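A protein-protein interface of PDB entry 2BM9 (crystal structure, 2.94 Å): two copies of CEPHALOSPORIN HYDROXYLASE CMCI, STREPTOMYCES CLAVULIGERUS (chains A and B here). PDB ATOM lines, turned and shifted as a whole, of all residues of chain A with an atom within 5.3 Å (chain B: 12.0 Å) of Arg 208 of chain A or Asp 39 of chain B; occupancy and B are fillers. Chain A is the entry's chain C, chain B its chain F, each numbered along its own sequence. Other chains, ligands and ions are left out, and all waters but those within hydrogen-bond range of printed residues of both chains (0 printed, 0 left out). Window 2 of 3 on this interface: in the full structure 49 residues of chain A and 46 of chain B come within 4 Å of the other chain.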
ATOM      1  N   LEU A 204      24.320  10.479 -27.646  1.00  0.00           N
ATOM      2  CA  LEU A 204      24.101  11.057 -26.321  1.00  0.00           C
ATOM      3  C   LEU A 204      23.475  10.006 -25.461  1.00  0.00           C
ATOM      4  O   LEU A 204      23.960   9.718 -24.366  1.00  0.00           O
ATOM      5  CB  LEU A 204      23.169  12.272 -26.393  1.00  0.00           C
ATOM      6  CG  LEU A 204      23.320  13.448 -25.415  1.00  0.00           C
ATOM      7  CD1 LEU A 204      21.937  13.883 -24.934  1.00  0.00           C
ATOM      8  CD2 LEU A 204      24.251  13.168 -24.241  1.00  0.00           C
ATOM      9  N   GLY A 205      22.392   9.431 -25.982  1.00  0.00           N
ATOM     10  CA  GLY A 205      21.698   8.316 -25.366  1.00  0.00           C
ATOM     11  C   GLY A 205      22.547   7.086 -25.126  1.00  0.00           C
ATOM     12  O   GLY A 205      22.184   6.253 -24.321  1.00  0.00           O
ATOM     13  N   ALA A 206      23.671   6.955 -25.813  1.00  0.00           N
ATOM     14  CA  ALA A 206      24.590   5.859 -25.538  1.00  0.00           C
ATOM     15  C   ALA A 206      25.200   5.929 -24.128  1.00  0.00           C
ATOM     16  O   ALA A 206      25.822   4.965 -23.660  1.00  0.00           O
ATOM     17  CB  ALA A 206      25.685   5.844 -26.574  1.00  0.00           C
ATOM     18  N   PHE A 207      25.034   7.079 -23.470  1.00  0.00           N
ATOM     19  CA  PHE A 207      25.575   7.328 -22.135  1.00  0.00           C
ATOM     20  C   PHE A 207      24.475   7.322 -21.094  1.00  0.00           C
ATOM     21  O   PHE A 207      24.721   7.626 -19.933  1.00  0.00           O
ATOM     22  CB  PHE A 207      26.257   8.701 -22.082  1.00  0.00           C
ATOM     23  CG  PHE A 207      27.505   8.804 -22.911  1.00  0.00           C
ATOM     24  CD1 PHE A 207      27.427   9.072 -24.270  1.00  0.00           C
ATOM     25  CD2 PHE A 207      28.758   8.676 -22.326  1.00  0.00           C
ATOM     26  CE1 PHE A 207      28.584   9.191 -25.037  1.00  0.00           C
ATOM     27  CE2 PHE A 207      29.918   8.801 -23.082  1.00  0.00           C
ATOM     28  CZ  PHE A 207      29.837   9.057 -24.432  1.00  0.00           C
ATOM     29  N   ARG A 208      23.257   6.987 -21.504  1.00  0.00           N
ATOM     30  CA  ARG A 208      22.114   7.077 -20.608  1.00  0.00           C
ATOM     31  C   ARG A 208      22.466   6.421 -19.294  1.00  0.00           C
ATOM     32  O   ARG A 208      22.195   6.998 -18.252  1.00  0.00           O
ATOM     33  CB  ARG A 208      20.851   6.454 -21.219  1.00  0.00           C
ATOM     34  CG  ARG A 208      20.766   4.917 -21.167  1.00  0.00           C
ATOM     35  CD  ARG A 208      19.852   4.292 -22.235  1.00  0.00           C
ATOM     36  NE  ARG A 208      20.623   3.951 -23.430  1.00  0.00           N
ATOM     37  CZ  ARG A 208      21.419   2.883 -23.551  1.00  0.00           C
ATOM     38  NH1 ARG A 208      21.546   1.989 -22.565  1.00  0.00           N
ATOM     39  NH2 ARG A 208      22.091   2.706 -24.684  1.00  0.00           N
ATOM     40  N   ASP A 209      23.120   5.255 -19.351  1.00  0.00           N
ATOM     41  CA  ASP A 209      23.448   4.473 -18.151  1.00  0.00           C
ATOM     42  C   ASP A 209      24.337   5.228 -17.154  1.00  0.00           C
ATOM     43  O   ASP A 209      24.150   5.116 -15.955  1.00  0.00           O
ATOM     44  CB  ASP A 209      24.102   3.123 -18.529  1.00  0.00           C
ATOM     45  CG  ASP A 209      23.080   2.077 -19.038  1.00  0.00           C
ATOM     46  OD1 ASP A 209      21.877   2.189 -18.725  1.00  0.00           O
ATOM     47  OD2 ASP A 209      23.397   1.106 -19.763  1.00  0.00           O
ATOM     48  N   VAL A 210      25.290   6.010 -17.648  1.00  0.00           N
ATOM     49  CA  VAL A 210      26.206   6.748 -16.772  1.00  0.00           C
ATOM     50  C   VAL A 210      25.854   8.226 -16.519  1.00  0.00           C
ATOM     51  O   VAL A 210      25.882   8.648 -15.372  1.00  0.00           O
ATOM     52  CB  VAL A 210      27.664   6.630 -17.270  1.00  0.00           C
ATOM     53  CG1 VAL A 210      28.024   5.159 -17.532  1.00  0.00           C
ATOM     54  CG2 VAL A 210      27.891   7.483 -18.519  1.00  0.00           C
ATOM     55  N   LEU A 211      25.517   8.996 -17.559  1.00  0.00           N
ATOM     56  CA  LEU A 211      25.344  10.466 -17.446  1.00  0.00           C
ATOM     57  C   LEU A 211      23.886  10.940 -17.553  1.00  0.00           C
ATOM     58  O   LEU A 211      23.084  10.337 -18.261  1.00  0.00           O
ATOM     59  CB  LEU A 211      26.165  11.184 -18.532  1.00  0.00           C
ATOM     60  CG  LEU A 211      27.647  11.509 -18.282  1.00  0.00           C
ATOM     61  CD1 LEU A 211      28.290  11.989 -19.566  1.00  0.00           C
ATOM     62  CD2 LEU A 211      27.830  12.546 -17.193  1.00  0.00           C
ATOM     63  N   PRO B  33      12.469  15.482 -12.942  1.00  0.00           N
ATOM     64  CA  PRO B  33      13.589  15.010 -12.136  1.00  0.00           C
ATOM     65  C   PRO B  33      14.812  15.843 -12.477  1.00  0.00           C
ATOM     66  O   PRO B  33      14.983  16.205 -13.639  1.00  0.00           O
ATOM     67  CB  PRO B  33      13.757  13.553 -12.587  1.00  0.00           C
ATOM     68  CG  PRO B  33      13.288  13.529 -13.987  1.00  0.00           C
ATOM     69  CD  PRO B  33      12.265  14.633 -14.128  1.00  0.00           C
ATOM     70  N   ARG B  34      15.622  16.173 -11.480  1.00  0.00           N
ATOM     71  CA  ARG B  34      16.896  16.816 -11.732  1.00  0.00           C
ATOM     72  C   ARG B  34      17.660  16.003 -12.765  1.00  0.00           C
ATOM     73  O   ARG B  34      18.132  16.549 -13.766  1.00  0.00           O
ATOM     74  CB  ARG B  34      17.716  16.927 -10.453  1.00  0.00           C
ATOM     75  CG  ARG B  34      18.082  18.343 -10.089  1.00  0.00           C
ATOM     76  CD  ARG B  34      19.055  18.429  -8.942  1.00  0.00           C
ATOM     77  NE  ARG B  34      20.214  19.258  -9.266  1.00  0.00           N
ATOM     78  CZ  ARG B  34      21.470  19.006  -8.895  1.00  0.00           C
ATOM     79  NH1 ARG B  34      21.775  17.930  -8.171  1.00  0.00           N
ATOM     80  NH2 ARG B  34      22.440  19.843  -9.251  1.00  0.00           N
ATOM     81  N   ASP B  35      17.763  14.696 -12.524  1.00  0.00           N
ATOM     82  CA  ASP B  35      18.455  13.791 -13.446  1.00  0.00           C
ATOM     83  C   ASP B  35      17.532  13.341 -14.568  1.00  0.00           C
ATOM     84  O   ASP B  35      16.860  12.312 -14.440  1.00  0.00           O
ATOM     85  CB  ASP B  35      18.982  12.553 -12.713  1.00  0.00           C
ATOM     86  CG  ASP B  35      19.972  12.895 -11.629  1.00  0.00           C
ATOM     87  OD1 ASP B  35      20.761  13.853 -11.821  1.00  0.00           O
ATOM     88  OD2 ASP B  35      20.027  12.249 -10.550  1.00  0.00           O
ATOM     89  N   TRP B  36      17.501  14.111 -15.660  1.00  0.00           N
ATOM     90  CA  TRP B  36      16.746  13.730 -16.851  1.00  0.00           C
ATOM     91  C   TRP B  36      17.496  12.602 -17.559  1.00  0.00           C
ATOM     92  O   TRP B  36      18.704  12.660 -17.682  1.00  0.00           O
ATOM     93  CB  TRP B  36      16.530  14.934 -17.783  1.00  0.00           C
ATOM     94  CG  TRP B  36      15.396  14.718 -18.751  1.00  0.00           C
ATOM     95  CD1 TRP B  36      15.482  14.160 -19.985  1.00  0.00           C
ATOM     96  CD2 TRP B  36      14.003  15.025 -18.549  1.00  0.00           C
ATOM     97  NE1 TRP B  36      14.239  14.103 -20.564  1.00  0.00           N
ATOM     98  CE2 TRP B  36      13.314  14.624 -19.701  1.00  0.00           C
ATOM     99  CE3 TRP B  36      13.266  15.592 -17.502  1.00  0.00           C
ATOM    100  CZ2 TRP B  36      11.934  14.774 -19.839  1.00  0.00           C
ATOM    101  CZ3 TRP B  36      11.889  15.744 -17.648  1.00  0.00           C
ATOM    102  CH2 TRP B  36      11.246  15.338 -18.802  1.00  0.00           C
ATOM    103  N   PRO B  37      16.812  11.550 -17.991  1.00  0.00           N
ATOM    104  CA  PRO B  37      17.503  10.490 -18.723  1.00  0.00           C
ATOM    105  C   PRO B  37      17.898  11.005 -20.101  1.00  0.00           C
ATOM    106  O   PRO B  37      17.085  11.647 -20.772  1.00  0.00           O
ATOM    107  CB  PRO B  37      16.471   9.363 -18.798  1.00  0.00           C
ATOM    108  CG  PRO B  37      15.161  10.018 -18.631  1.00  0.00           C
ATOM    109  CD  PRO B  37      15.375  11.272 -17.838  1.00  0.00           C
ATOM    110  N   LEU B  38      19.143  10.752 -20.493  1.00  0.00           N
ATOM    111  CA  LEU B  38      19.697  11.295 -21.736  1.00  0.00           C
ATOM    112  C   LEU B  38      19.051  10.711 -22.982  1.00  0.00           C
ATOM    113  O   LEU B  38      18.865  11.412 -23.969  1.00  0.00           O
ATOM    114  CB  LEU B  38      21.203  11.049 -21.792  1.00  0.00           C
ATOM    115  CG  LEU B  38      22.126  12.264 -21.680  1.00  0.00           C
ATOM    116  CD1 LEU B  38      21.586  13.379 -20.771  1.00  0.00           C
ATOM    117  CD2 LEU B  38      23.516  11.785 -21.215  1.00  0.00           C
ATOM    118  N   ASP B  39      18.713   9.424 -22.928  1.00  0.00           N
ATOM    119  CA  ASP B  39      18.052   8.743 -24.046  1.00  0.00           C
ATOM    120  C   ASP B  39      16.660   9.301 -24.371  1.00  0.00           C
ATOM    121  O   ASP B  39      16.017   8.838 -25.308  1.00  0.00           O
ATOM    122  CB  ASP B  39      17.962   7.228 -23.792  1.00  0.00           C
ATOM    123  CG  ASP B  39      17.050   6.896 -22.664  1.00  0.00           C
ATOM    124  OD1 ASP B  39      16.740   7.816 -21.877  1.00  0.00           O
ATOM    125  OD2 ASP B  39      16.596   5.749 -22.476  1.00  0.00           O
ATOM    126  N   ARG B  40      16.194  10.272 -23.592  1.00  0.00           N
ATOM    127  CA  ARG B  40      14.991  11.020 -23.930  1.00  0.00           C
ATOM    128  C   ARG B  40      15.346  12.505 -23.964  1.00  0.00           C
ATOM    129  O   ARG B  40      14.627  13.342 -23.429  1.00  0.00           O
ATOM    130  CB  ARG B  40      13.867  10.710 -22.929  1.00  0.00           C
ATOM    131  CG  ARG B  40      13.869   9.246 -22.417  1.00  0.00           C
ATOM    132  CD  ARG B  40      12.593   8.798 -21.709  1.00  0.00           C
ATOM    133  NE  ARG B  40      11.530   8.457 -22.654  1.00  0.00           N
ATOM    134  CZ  ARG B  40      10.230   8.575 -22.410  1.00  0.00           C
ATOM    135  NH1 ARG B  40       9.811   9.030 -21.231  1.00  0.00           N
ATOM    136  NH2 ARG B  40       9.343   8.244 -23.350  1.00  0.00           N
ATOM    137  N   TRP B  41      16.451  12.826 -24.638  1.00  0.00           N
ATOM    138  CA  TRP B  41      17.010  14.169 -24.574  1.00  0.00           C
ATOM    139  C   TRP B  41      16.020  15.170 -25.140  1.00  0.00           C
ATOM    140  O   TRP B  41      15.672  16.129 -24.465  1.00  0.00           O
ATOM    141  CB  TRP B  41      18.372  14.277 -25.289  1.00  0.00           C
ATOM    142  CG  TRP B  41      18.995  15.680 -25.209  1.00  0.00           C
ATOM    143  CD1 TRP B  41      19.825  16.158 -24.236  1.00  0.00           C
ATOM    144  CD2 TRP B  41      18.812  16.761 -26.140  1.00  0.00           C
ATOM    145  NE1 TRP B  41      20.162  17.464 -24.499  1.00  0.00           N
ATOM    146  CE2 TRP B  41      19.552  17.860 -25.661  1.00  0.00           C
ATOM    147  CE3 TRP B  41      18.077  16.917 -27.325  1.00  0.00           C
ATOM    148  CZ2 TRP B  41      19.585  19.097 -26.330  1.00  0.00           C
ATOM    149  CZ3 TRP B  41      18.110  18.150 -27.990  1.00  0.00           C
ATOM    150  CH2 TRP B  41      18.858  19.219 -27.488  1.00  0.00           C
ATOM    151  N   ALA B  42      15.552  14.949 -26.365  1.00  0.00           N
ATOM    152  CA  ALA B  42      14.679  15.934 -27.019  1.00  0.00           C
ATOM    153  C   ALA B  42      13.364  16.086 -26.237  1.00  0.00           C
ATOM    154  O   ALA B  42      12.743  17.158 -26.224  1.00  0.00           O
ATOM    155  CB  ALA B  42      14.413  15.537 -28.482  1.00  0.00           C
ATOM    156  N   GLU B  43      12.982  15.010 -25.552  1.00  0.00           N
ATOM    157  CA  GLU B  43      11.710  14.923 -24.857  1.00  0.00           C
ATOM    158  C   GLU B  43      11.596  15.871 -23.660  1.00  0.00           C
ATOM    159  O   GLU B  43      10.498  16.067 -23.138  1.00  0.00           O
ATOM    160  CB  GLU B  43      11.498  13.482 -24.390  1.00  0.00           C
ATOM    161  CG  GLU B  43      10.370  12.736 -25.079  1.00  0.00           C
ATOM    162  CD  GLU B  43      10.052  11.410 -24.384  1.00  0.00           C
ATOM    163  OE1 GLU B  43       9.463  11.417 -23.269  1.00  0.00           O
ATOM    164  OE2 GLU B  43      10.404  10.351 -24.951  1.00  0.00           O
ATOM    165  N   ALA B  44      12.715  16.459 -23.236  1.00  0.00           N
ATOM    166  CA  ALA B  44      12.787  17.260 -22.007  1.00  0.00           C
ATOM    167  C   ALA B  44      12.422  18.742 -22.171  1.00  0.00           C
ATOM    168  O   ALA B  44      12.795  19.397 -23.151  1.00  0.00           O
ATOM    169  CB  ALA B  44      14.169  17.159 -21.416  1.00  0.00           C
ATOM    170  N   PRO B  45      11.743  19.277 -21.163  1.00  0.00           N
ATOM    171  CA  PRO B  45      11.173  20.625 -21.240  1.00  0.00           C
ATOM    172  C   PRO B  45      12.268  21.657 -21.226  1.00  0.00           C
ATOM    173  O   PRO B  45      13.326  21.408 -20.636  1.00  0.00           O
ATOM    174  CB  PRO B  45      10.342  20.720 -19.964  1.00  0.00           C
ATOM    175  CG  PRO B  45      11.041  19.808 -19.019  1.00  0.00           C
ATOM    176  CD  PRO B  45      11.513  18.658 -19.848  1.00  0.00           C
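The backbone carbonyl oxygen of Gly 205 of chain A lies within hydrogen-bond range of the guanidinium group of Arg 208 of chain A. The guanidinium group (NH1) of Arg 208 of chain A is in salt-bridge range of the side-chain carboxylate (OD2) of Asp 209 of chain A.
Leu 204 of chain A touches Leu 38 of chain B. CD1 of Trp 41 of chain B touches CD1 of Leu 204 of chain A (3.2 Å). Gly 205 of chain A touches Asp 39 of chain B. Asp 39 of chain B touches Arg 208 of chain A (OD2 to CD, 3.6 Å). Leu 38 of chain B touches Leu 211 of chain A (CD2 to O, 3.3 Å).
Of the printed residues of chain B, Arg 208 of chain A touches Asp 39. Of chain A, only Gly 205 and Arg 208 come within 4 Å of Asp 39 of chain B. Gly 205 of chain A touches just one residue of chain B: Asp 39 (3.9 Å). Ala 206 of chain A touches none of the printed residues of chain B. No residue of chain B comes within 4 Å of Phe 207 of chain A. No residue of chain B comes within 4 Å of Val 210 of chain A. Printed residues of chain A within 4 Å of Leu 38 of chain B: Leu 204 (3.4 Å) and Leu 211 (3.3 Å). Printed residues of chain B within 4 Å of Leu 211 of chain A: Leu 38 (3.3 Å). Printed residues of chain A within 4 Å of Trp 41 of chain B: Leu 204 (3.2 Å). Asp 35 of chain B touches none of the printed residues of chain A. The nearest printed residue of chain A that does not touch Asp 39 of chain B is Leu 204 of chain A (5.4 Å).
Of the 8 printed residues of chain A, 4 touch a printed residue of chain B. Hydrophobic or aromatic side chains of chain A within 4 Å of the printed part of chain B: Leu 204 and Leu 211. Among the printed residues, 5 pairs touch across the chains.
No position is printed for both chains. Of the 5 pairs that touch across the chains among the printed residues, none has its exchanged pair printed and touching as well.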
